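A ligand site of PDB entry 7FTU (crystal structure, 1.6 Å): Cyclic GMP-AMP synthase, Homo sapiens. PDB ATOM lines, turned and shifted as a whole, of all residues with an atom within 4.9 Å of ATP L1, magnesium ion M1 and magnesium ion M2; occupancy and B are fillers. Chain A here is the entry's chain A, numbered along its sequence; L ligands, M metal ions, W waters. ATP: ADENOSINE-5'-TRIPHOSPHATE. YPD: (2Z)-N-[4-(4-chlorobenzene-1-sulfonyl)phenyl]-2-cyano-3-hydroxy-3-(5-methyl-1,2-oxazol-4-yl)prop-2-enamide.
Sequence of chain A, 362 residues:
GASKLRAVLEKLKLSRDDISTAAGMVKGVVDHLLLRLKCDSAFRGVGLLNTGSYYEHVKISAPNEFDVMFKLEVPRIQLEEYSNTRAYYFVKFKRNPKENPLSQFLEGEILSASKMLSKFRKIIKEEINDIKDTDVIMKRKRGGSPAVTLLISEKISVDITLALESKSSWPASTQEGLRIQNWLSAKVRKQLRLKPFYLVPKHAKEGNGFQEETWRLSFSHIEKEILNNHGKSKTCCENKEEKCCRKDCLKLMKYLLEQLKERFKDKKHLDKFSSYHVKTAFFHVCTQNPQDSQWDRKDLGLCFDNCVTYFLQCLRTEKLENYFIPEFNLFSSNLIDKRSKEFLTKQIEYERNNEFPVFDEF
The side-chain hydroxyl (OG) of Ser 53 is in hydrogen-bond range of an oxygen (O3G) of ATP L1.
An oxygen (O3G) of ATP L1 is in salt-bridge range of the side-chain amino group of Lys 254, at 2.9 Å.
OG of Ser 275 sits at hydrogen-bond distance from O2G of ATP L1 (2.7 Å).
The side-chain hydroxyl of Ser 220 is in hydrogen-bond range of an oxygen (O2') of ATP L1, 2.5 Å away.
N3 of ATP L1 lies close to NH1 of Arg 216 (3.5 Å).
The side-chain carboxylate (OE1) of Glu 223 lies within hydrogen-bond range of an oxygen (O2') of ATP L1, at 2.6 Å.
The side-chain amino group (NZ) of Lys 279 lies within hydrogen-bond range of an oxygen (O3') of ATP L1 (2.9 Å).
An oxygen (O2) of YPD L2 lies within hydrogen-bond range of the guanidinium group (NH2) of Arg 216.
The backbone NH (N) of Ser 53 sits close to an oxygen (O2B) of ATP L1, at 3.0 Å.
An oxygen (O4') of ATP L1 sits close to an oxygen (O7) of YPD L2.
The side-chain hydroxyl (OH) of Tyr 276 sits at hydrogen-bond distance from the side-chain carboxylate (OE2) of Glu 223 (2.7 Å).
The backbone NH (N) of Lys 59 sits at hydrogen-bond distance from the backbone carbonyl oxygen (O) of Ser 53, at 3.1 Å.
The side-chain carboxylate (OE1) of Glu 223 is in salt-bridge range of the side-chain amino group (NZ) of Lys 279, at 2.7 Å.
NZ of Lys 279 lies within salt-bridge range of OE2 of Glu 56 (2.6 Å).
The backbone NH (N) of Asp 159 is in hydrogen-bond range of the backbone carbonyl oxygen (O) of Phe 66 (2.8 Å).
Gly 52 touches ATP L1.
Lys 59 touches ATP L1.
CE2 of Tyr 276 touches N1 of ATP L1 (3.4 Å).
Hydrophobic or aromatic side chains that line ATP L1: Tyr 276.
12 residues have an atom within 4 Å of ATP L1: Gly 52, Ser 53, Lys 59, Glu 65, Asp 67, Arg 216, Ser 220, Glu 223, Lys 254, Ser 275, Tyr 276 and Lys 279.
Along chain A the residues within 4 Å of ATP L1 span positions 52 to 279.
Within 4 Å of magnesium ion M1: Glu 65 and Asp 67.
The nearest printed residue that does not touch magnesium ion M1 is Ser 53 (4.02 Å).
Of the 18 residues printed, 3 come within 4 Å of magnesium ion M2.
Along chain A the residues within 4 Å of magnesium ion M2 span positions 65 to 159.
Magnesium ion M1 is bound by the side-chain carboxylate (OD2) of Asp 67 (2.0 Å), an oxygen (O1G) of ATP L1 (2.0 Å), an oxygen (O2B) of ATP L1 (2.0 Å), the side-chain carboxylate (OE1) of Glu 65 (2.0 Å), an oxygen (O2A) of ATP L1 (2.0 Å) and water W1 (2.2 Å).
Magnesium ion M1 has six donor atoms within binding distance.
Magnesium ion M2 is bound by water W5, OD1 of Asp 67, OE2 of Glu 65, OD2 of Asp 159, water W2 and O2A of ATP L1.
Water W2 lies within hydrogen-bond range of O7 of YPD L2 (2.8 Å) and O5' of ATP L1 (3.1 Å).
Water W7 lies within hydrogen-bond range of an oxygen (O1B) of ATP L1 (2.7 Å) and the side-chain carboxylate (OE1) of Glu 56 (2.7 Å).
Water W13 lies within hydrogen-bond range of N1 of ATP L1 (2.8 Å) and ND2 of Asn 322 (2.9 Å).
Water W14 lies within hydrogen-bond range of an oxygen (O1A) of ATP L1, the side-chain hydroxyl of Ser 275 and the backbone NH of Tyr 276.
Water W3 lies within hydrogen-bond range of OE2 of Glu 223 (2.8 Å), N3 of ATP L1 (3.2 Å) and OH of Tyr 276 (3.5 Å).
Water W4 lies within hydrogen-bond range of the side-chain amino group of Lys 254 (2.7 Å) and an oxygen (O2G) of ATP L1 (3.3 Å).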
ATOM      1  N   GLY A  52       7.929  13.314  -0.347  1.00  0.00           N
ATOM      2  CA  GLY A  52       6.638  13.886  -0.668  1.00  0.00           C
ATOM      3  C   GLY A  52       5.510  13.427   0.258  1.00  0.00           C
ATOM      4  O   GLY A  52       5.748  12.757   1.275  1.00  0.00           O
ATOM      5  N   SER A  53       4.277  13.754  -0.120  1.00  0.00           N
ATOM      6  CA  SER A  53       3.185  13.856   0.840  1.00  0.00           C
ATOM      7  C   SER A  53       2.752  12.483   1.328  1.00  0.00           C
ATOM      8  O   SER A  53       2.295  12.350   2.470  1.00  0.00           O
ATOM      9  CB  SER A  53       2.025  14.625   0.266  1.00  0.00           C
ATOM     10  OG  SER A  53       1.445  13.953  -0.829  1.00  0.00           O
ATOM     11  N   GLU A  56       5.114  11.532   4.070  1.00  0.00           N
ATOM     12  CA  GLU A  56       5.018  12.527   5.117  1.00  0.00           C
ATOM     13  C   GLU A  56       3.653  12.460   5.806  1.00  0.00           C
ATOM     14  O   GLU A  56       3.390  13.198   6.750  1.00  0.00           O
ATOM     15  CB  GLU A  56       5.190  13.922   4.502  1.00  0.00           C
ATOM     16  CG  GLU A  56       6.583  14.203   3.952  1.00  0.00           C
ATOM     17  CD  GLU A  56       6.669  15.400   3.021  1.00  0.00           C
ATOM     18  OE1 GLU A  56       5.636  15.762   2.428  1.00  0.00           O
ATOM     19  OE2 GLU A  56       7.772  15.995   2.912  1.00  0.00           O
ATOM     20  N   LYS A  59      -0.631  13.423   2.424  1.00  0.00           N
ATOM     21  CA  LYS A  59      -1.399  13.200   1.215  1.00  0.00           C
ATOM     22  C   LYS A  59      -2.885  13.237   1.573  1.00  0.00           C
ATOM     23  O   LYS A  59      -3.277  12.651   2.585  1.00  0.00           O
ATOM     24  CB  LYS A  59      -1.052  11.823   0.630  1.00  0.00           C
ATOM     25  CG  LYS A  59      -1.708  11.510  -0.703  1.00  0.00           C
ATOM     26  CD  LYS A  59      -1.060  12.245  -1.848  1.00  0.00           C
ATOM     27  CE  LYS A  59      -1.802  12.088  -3.164  1.00  0.00           C
ATOM     28  NZ  LYS A  59      -3.162  12.664  -3.094  1.00  0.00           N
ATOM     29  N   GLU A  65      -0.673   9.610  -5.770  1.00  0.00           N
ATOM     30  CA  GLU A  65       0.489  10.341  -6.277  1.00  0.00           C
ATOM     31  C   GLU A  65       1.637  10.165  -5.276  1.00  0.00           C
ATOM     32  O   GLU A  65       1.555  10.560  -4.112  1.00  0.00           O
ATOM     33  CB  GLU A  65       0.159  11.805  -6.599  1.00  0.00           C
ATOM     34  CG  GLU A  65       1.208  12.522  -7.467  1.00  0.00           C
ATOM     35  CD  GLU A  65       2.390  13.228  -6.796  1.00  0.00           C
ATOM     36  OE1 GLU A  65       2.443  13.241  -5.561  1.00  0.00           O
ATOM     37  OE2 GLU A  65       3.256  13.788  -7.513  1.00  0.00           O
ATOM     38  N   PHE A  66       2.683   9.478  -5.777  1.00  0.00           N
ATOM     39  CA  PHE A  66       3.881   9.158  -5.024  1.00  0.00           C
ATOM     40  C   PHE A  66       5.060   9.883  -5.660  1.00  0.00           C
ATOM     41  O   PHE A  66       5.093  10.087  -6.878  1.00  0.00           O
ATOM     42  CB  PHE A  66       4.199   7.661  -5.058  1.00  0.00           C
ATOM     43  CG  PHE A  66       3.199   6.779  -4.354  1.00  0.00           C
ATOM     44  CD1 PHE A  66       1.910   6.626  -4.853  1.00  0.00           C
ATOM     45  CD2 PHE A  66       3.542   6.099  -3.201  1.00  0.00           C
ATOM     46  CE1 PHE A  66       0.999   5.814  -4.211  1.00  0.00           C
ATOM     47  CE2 PHE A  66       2.625   5.292  -2.553  1.00  0.00           C
ATOM     48  CZ  PHE A  66       1.356   5.142  -3.066  1.00  0.00           C
ATOM     49  N   ASP A  67       6.026  10.222  -4.803  1.00  0.00           N
ATOM     50  CA  ASP A  67       7.237  10.877  -5.232  1.00  0.00           C
ATOM     51  C   ASP A  67       8.413  10.068  -4.690  1.00  0.00           C
ATOM     52  O   ASP A  67       8.405   9.682  -3.514  1.00  0.00           O
ATOM     53  CB  ASP A  67       7.273  12.329  -4.750  1.00  0.00           C
ATOM     54  CG  ASP A  67       6.057  13.114  -5.180  1.00  0.00           C
ATOM     55  OD1 ASP A  67       6.048  13.604  -6.341  1.00  0.00           O
ATOM     56  OD2 ASP A  67       5.111  13.242  -4.336  1.00  0.00           O
ATOM     57  N   ASP A 159       5.965  10.213  -9.565  1.00  0.00           N
ATOM     58  CA  ASP A 159       7.032  11.095 -10.013  1.00  0.00           C
ATOM     59  C   ASP A 159       8.342  10.500  -9.553  1.00  0.00           C
ATOM     60  O   ASP A 159       8.548  10.288  -8.357  1.00  0.00           O
ATOM     61  CB  ASP A 159       6.883  12.514  -9.451  1.00  0.00           C
ATOM     62  CG  ASP A 159       5.680  13.295  -9.964  1.00  0.00           C
ATOM     63  OD1 ASP A 159       5.186  12.951 -11.083  1.00  0.00           O
ATOM     64  OD2 ASP A 159       5.240  14.217  -9.226  1.00  0.00           O
ATOM     65  N   ARG A 216      19.082  21.856  -9.709  1.00  0.00           N
ATOM     66  CA  ARG A 216      18.538  22.594  -8.580  1.00  0.00           C
ATOM     67  C   ARG A 216      18.663  21.786  -7.288  1.00  0.00           C
ATOM     68  O   ARG A 216      18.494  20.566  -7.296  1.00  0.00           O
ATOM     69  CB  ARG A 216      17.065  22.943  -8.796  1.00  0.00           C
ATOM     70  CG  ARG A 216      16.626  24.166  -8.000  1.00  0.00           C
ATOM     71  CD  ARG A 216      15.153  24.170  -7.652  1.00  0.00           C
ATOM     72  NE  ARG A 216      14.887  23.050  -6.774  1.00  0.00           N
ATOM     73  CZ  ARG A 216      13.962  22.118  -6.988  1.00  0.00           C
ATOM     74  NH1 ARG A 216      13.967  21.018  -6.256  1.00  0.00           N
ATOM     75  NH2 ARG A 216      13.078  22.254  -7.958  1.00  0.00           N
ATOM     76  N   LEU A 217      18.940  22.471  -6.176  1.00  0.00           N
ATOM     77  CA  LEU A 217      19.020  21.808  -4.883  1.00  0.00           C
ATOM     78  C   LEU A 217      17.659  21.238  -4.500  1.00  0.00           C
ATOM     79  O   LEU A 217      16.617  21.825  -4.818  1.00  0.00           O
ATOM     80  CB  LEU A 217      19.475  22.806  -3.802  1.00  0.00           C
ATOM     81  CG  LEU A 217      20.917  23.272  -3.896  1.00  0.00           C
ATOM     82  CD1 LEU A 217      21.159  24.431  -2.939  1.00  0.00           C
ATOM     83  CD2 LEU A 217      21.868  22.144  -3.587  1.00  0.00           C
ATOM     84  N   SER A 220      14.150  17.356  -0.070  1.00  0.00           N
ATOM     85  CA  SER A 220      12.925  16.595   0.161  1.00  0.00           C
ATOM     86  C   SER A 220      13.068  15.631   1.332  1.00  0.00           C
ATOM     87  O   SER A 220      12.078  15.324   2.014  1.00  0.00           O
ATOM     88  CB  SER A 220      12.519  15.842  -1.083  1.00  0.00           C
ATOM     89  OG  SER A 220      12.185  16.740  -2.136  1.00  0.00           O
ATOM     90  N   GLU A 223      12.665  17.685   4.538  1.00  0.00           N
ATOM     91  CA  GLU A 223      11.254  18.034   4.671  1.00  0.00           C
ATOM     92  C   GLU A 223      10.477  16.874   5.270  1.00  0.00           C
ATOM     93  O   GLU A 223       9.627  17.048   6.147  1.00  0.00           O
ATOM     94  CB  GLU A 223      10.669  18.444   3.312  1.00  0.00           C
ATOM     95  CG  GLU A 223      11.331  19.680   2.746  1.00  0.00           C
ATOM     96  CD  GLU A 223      10.925  20.056   1.338  1.00  0.00           C
ATOM     97  OE1 GLU A 223      10.001  19.424   0.797  1.00  0.00           O
ATOM     98  OE2 GLU A 223      11.564  20.982   0.781  1.00  0.00           O
ATOM     99  N   LYS A 254      -3.548  22.574   1.693  1.00  0.00           N
ATOM    100  CA  LYS A 254      -3.400  21.879   0.424  1.00  0.00           C
ATOM    101  C   LYS A 254      -4.757  21.762  -0.276  1.00  0.00           C
ATOM    102  O   LYS A 254      -4.841  22.016  -1.477  1.00  0.00           O
ATOM    103  CB  LYS A 254      -2.801  20.482   0.626  1.00  0.00           C
ATOM    104  CG  LYS A 254      -1.331  20.477   0.995  1.00  0.00           C
ATOM    105  CD  LYS A 254      -0.811  19.157   1.535  1.00  0.00           C
ATOM    106  CE  LYS A 254      -0.830  18.022   0.530  1.00  0.00           C
ATOM    107  NZ  LYS A 254      -0.176  18.433  -0.729  1.00  0.00           N
ATOM    108  N   SER A 275       1.252  22.794  -4.641  1.00  0.00           N
ATOM    109  CA  SER A 275       1.227  22.376  -3.256  1.00  0.00           C
ATOM    110  C   SER A 275       2.516  22.748  -2.534  1.00  0.00           C
ATOM    111  O   SER A 275       2.475  23.006  -1.331  1.00  0.00           O
ATOM    112  CB  SER A 275       0.912  20.897  -3.143  1.00  0.00           C
ATOM    113  OG  SER A 275       1.978  20.102  -3.618  1.00  0.00           O
ATOM    114  N   TYR A 276       3.666  22.794  -3.234  1.00  0.00           N
ATOM    115  CA  TYR A 276       4.927  23.123  -2.574  1.00  0.00           C
ATOM    116  C   TYR A 276       4.911  24.558  -2.033  1.00  0.00           C
ATOM    117  O   TYR A 276       5.631  24.880  -1.075  1.00  0.00           O
ATOM    118  CB  TYR A 276       6.133  22.924  -3.501  1.00  0.00           C
ATOM    119  CG  TYR A 276       7.467  22.981  -2.792  1.00  0.00           C
ATOM    120  CD1 TYR A 276       7.799  22.054  -1.818  1.00  0.00           C
ATOM    121  CD2 TYR A 276       8.374  24.004  -3.023  1.00  0.00           C
ATOM    122  CE1 TYR A 276       8.997  22.117  -1.125  1.00  0.00           C
ATOM    123  CE2 TYR A 276       9.572  24.091  -2.333  1.00  0.00           C
ATOM    124  CZ  TYR A 276       9.894  23.134  -1.378  1.00  0.00           C
ATOM    125  OH  TYR A 276      11.078  23.165  -0.676  1.00  0.00           O
ATOM    126  N   LYS A 279       3.156  24.124   1.266  1.00  0.00           N
ATOM    127  CA  LYS A 279       4.083  23.420   2.143  1.00  0.00           C
ATOM    128  C   LYS A 279       5.147  24.370   2.690  1.00  0.00           C
ATOM    129  O   LYS A 279       5.430  24.345   3.883  1.00  0.00           O
ATOM    130  CB  LYS A 279       4.758  22.263   1.410  1.00  0.00           C
ATOM    131  CG  LYS A 279       5.449  21.245   2.305  1.00  0.00           C
ATOM    132  CD  LYS A 279       6.300  20.262   1.503  1.00  0.00           C
ATOM    133  CE  LYS A 279       6.844  19.105   2.322  1.00  0.00           C
ATOM    134  NZ  LYS A 279       7.690  18.207   1.512  1.00  0.00           N
ATOM    135  N   ASN A 322      12.149  30.021  -0.218  1.00  0.00           N
ATOM    136  CA  ASN A 322      12.467  28.623  -0.047  1.00  0.00           C
ATOM    137  C   ASN A 322      12.940  28.430   1.401  1.00  0.00           C
ATOM    138  O   ASN A 322      13.713  29.221   1.934  1.00  0.00           O
ATOM    139  CB  ASN A 322      13.484  28.209  -1.102  1.00  0.00           C
ATOM    140  CG  ASN A 322      13.881  26.755  -0.986  1.00  0.00           C
ATOM    141  OD1 ASN A 322      14.549  26.372  -0.028  1.00  0.00           O
ATOM    142  ND2 ASN A 322      13.527  25.946  -1.961  1.00  0.00           N
ATOM    143  N   LEU A 330      10.205  31.936  -4.286  1.00  0.00           N
ATOM    144  CA  LEU A 330       9.312  31.138  -5.110  1.00  0.00           C
ATOM    145  C   LEU A 330       8.227  32.009  -5.755  1.00  0.00           C
ATOM    146  O   LEU A 330       7.588  31.577  -6.722  1.00  0.00           O
ATOM    147  CB  LEU A 330       8.654  30.045  -4.255  1.00  0.00           C
ATOM    148  CG  LEU A 330       9.593  29.067  -3.528  1.00  0.00           C
ATOM    149  CD1 LEU A 330       8.801  28.078  -2.699  1.00  0.00           C
ATOM    150  CD2 LEU A 330      10.478  28.320  -4.503  1.00  0.00           C
HETATM  151  PG  ATP L   1       1.175  16.520  -3.138  1.00  0.00           P
HETATM  152  O1G ATP L   1       1.858  15.521  -4.056  1.00  0.00           O
HETATM  153  O2G ATP L   1       0.653  17.736  -3.813  1.00  0.00           O
HETATM  154  O3G ATP L   1       0.195  15.918  -2.172  1.00  0.00           O
HETATM  155  PB  ATP L   1       3.955  16.803  -2.389  1.00  0.00           P
HETATM  156  O1B ATP L   1       4.723  17.465  -1.271  1.00  0.00           O
HETATM  157  O2B ATP L   1       4.188  15.330  -2.651  1.00  0.00           O
HETATM  158  O3B ATP L   1       2.402  17.069  -2.222  1.00  0.00           O
HETATM  159  PA  ATP L   1       4.832  17.129  -5.166  1.00  0.00           P
HETATM  160  O1A ATP L   1       4.407  18.199  -6.122  1.00  0.00           O
HETATM  161  O2A ATP L   1       4.477  15.688  -5.496  1.00  0.00           O
HETATM  162  O3A ATP L   1       4.213  17.573  -3.762  1.00  0.00           O
HETATM  163  O5' ATP L   1       6.392  17.258  -4.877  1.00  0.00           O
HETATM  164  C5' ATP L   1       7.079  16.214  -4.165  1.00  0.00           C
HETATM  165  C4' ATP L   1       8.223  16.830  -3.411  1.00  0.00           C
HETATM  166  O4' ATP L   1       9.107  17.486  -4.356  1.00  0.00           O
HETATM  167  C3' ATP L   1       7.876  17.944  -2.427  1.00  0.00           C
HETATM  168  O3' ATP L   1       7.370  17.409  -1.211  1.00  0.00           O
HETATM  169  C2' ATP L   1       9.233  18.639  -2.297  1.00  0.00           C
HETATM  170  O2' ATP L   1      10.106  17.978  -1.413  1.00  0.00           O
HETATM  171  C1' ATP L   1       9.763  18.564  -3.729  1.00  0.00           C
HETATM  172  N9  ATP L   1       9.493  19.759  -4.520  1.00  0.00           N
HETATM  173  C8  ATP L   1       8.407  19.985  -5.328  1.00  0.00           C
HETATM  174  N7  ATP L   1       8.455  21.162  -5.898  1.00  0.00           N
HETATM  175  C5  ATP L   1       9.627  21.732  -5.428  1.00  0.00           C
HETATM  176  C6  ATP L   1      10.236  22.987  -5.664  1.00  0.00           C
HETATM  177  N6  ATP L   1       9.709  23.921  -6.451  1.00  0.00           N
HETATM  178  N1  ATP L   1      11.405  23.241  -5.041  1.00  0.00           N
HETATM  179  C2  ATP L   1      11.907  22.311  -4.217  1.00  0.00           C
HETATM  180  N3  ATP L   1      11.427  21.105  -3.916  1.00  0.00           N
HETATM  181  C4  ATP L   1      10.271  20.881  -4.567  1.00  0.00           C
HETATM  182  C13 YPD L   2       9.701  13.386  -7.535  1.00  0.00           C
HETATM  183  C15 YPD L   2       9.364  19.820  -9.410  1.00  0.00           C
HETATM  184  C16 YPD L   2       8.489  19.388 -10.395  1.00  0.00           C
HETATM  185  C17 YPD L   2       8.015  20.271 -11.351  1.00  0.00           C
HETATM  186  C18 YPD L   2       8.411  21.600 -11.306  1.00  0.00           C
HETATM  187  C19 YPD L   2       9.273  22.057 -10.322  1.00  0.00           C
HETATM  188  C20 YPD L   2       9.746  21.158  -9.370  1.00  0.00           C
HETATM  189  C22 YPD L   2       6.219  23.244 -11.988  1.00  0.00           C
HETATM  190  C23 YPD L   2       6.045  24.525 -11.491  1.00  0.00           C
HETATM  191  C24 YPD L   2       4.791  24.926 -11.064  1.00  0.00           C
HETATM  192  C25 YPD L   2       3.731  24.047 -11.147  1.00  0.00           C
HETATM  193  C26 YPD L   2       3.898  22.771 -11.637  1.00  0.00           C
HETATM  194  C27 YPD L   2       5.153  22.363 -12.058  1.00  0.00           C
HETATM  195  C1  YPD L   2      10.901  18.892  -7.650  1.00  0.00           C
HETATM  196  O2  YPD L   2      11.615  19.890  -7.516  1.00  0.00           O
HETATM  197  C3  YPD L   2      11.205  17.682  -6.878  1.00  0.00           C
HETATM  198  C4  YPD L   2      12.358  17.727  -6.051  1.00  0.00           C
HETATM  199  N5  YPD L   2      13.289  17.804  -5.404  1.00  0.00           N
HETATM  200  C6  YPD L   2      10.456  16.517  -6.882  1.00  0.00           C
HETATM  201  O7  YPD L   2       9.365  16.414  -7.627  1.00  0.00           O
HETATM  202  C8  YPD L   2      10.727  15.315  -6.084  1.00  0.00           C
HETATM  203  C9  YPD L   2      10.385  14.028  -6.389  1.00  0.00           C
HETATM  204  O10 YPD L   2      10.807  13.214  -5.411  1.00  0.00           O
HETATM  205  N11 YPD L   2      11.439  13.975  -4.401  1.00  0.00           N
HETATM  206  C12 YPD L   2      11.361  15.202  -4.829  1.00  0.00           C
HETATM  207  N14 YPD L   2       9.799  18.859  -8.466  1.00  0.00           N
HETATM  208  S21 YPD L   2       7.812  22.717 -12.535  1.00  0.00           S
HETATM  209 CL28 YPD L   2       2.155  24.543 -10.622  1.00  0.00          CL
HETATM  210  O29 YPD L   2       8.674  23.878 -12.542  1.00  0.00           O
HETATM  211  O30 YPD L   2       7.644  21.973 -13.751  1.00  0.00           O
HETATM  212 MG    MG M   1       3.484  14.382  -4.272  1.00  0.00          MG
HETATM  213 MG    MG M   2       4.930  14.915  -7.346  1.00  0.00          MG
HETATM  214  O   HOH W   1       2.667  12.812  -2.981  1.00  0.00           O
HETATM  215  O   HOH W   2       6.611  16.016  -7.684  1.00  0.00           O
HETATM  216  O   HOH W   3      13.337  20.633  -1.375  1.00  0.00           O
HETATM  217  O   HOH W   4      -1.998  19.162  -2.581  1.00  0.00           O
HETATM  218  O   HOH W   5       3.853  16.311  -8.242  1.00  0.00           O
HETATM  219  O   HOH W   6       6.674  24.188  -7.666  1.00  0.00           O
HETATM  220  O   HOH W   7       3.831  17.484   1.309  1.00  0.00           O
HETATM  221  O   HOH W   8       5.888  19.026  -8.325  1.00  0.00           O
HETATM  222  O   HOH W   9       6.258  21.688  -7.366  1.00  0.00           O
HETATM  223  O   HOH W  10       3.921  20.105  -1.646  1.00  0.00           O
HETATM  224  O   HOH W  11       0.535  15.498  -6.605  1.00  0.00           O
HETATM  225  O   HOH W  12      -2.341  15.320  -1.648  1.00  0.00           O
HETATM  226  O   HOH W  13      12.661  25.671  -4.705  1.00  0.00           O
HETATM  227  O   HOH W  14       4.110  20.954  -5.783  1.00  0.00           O
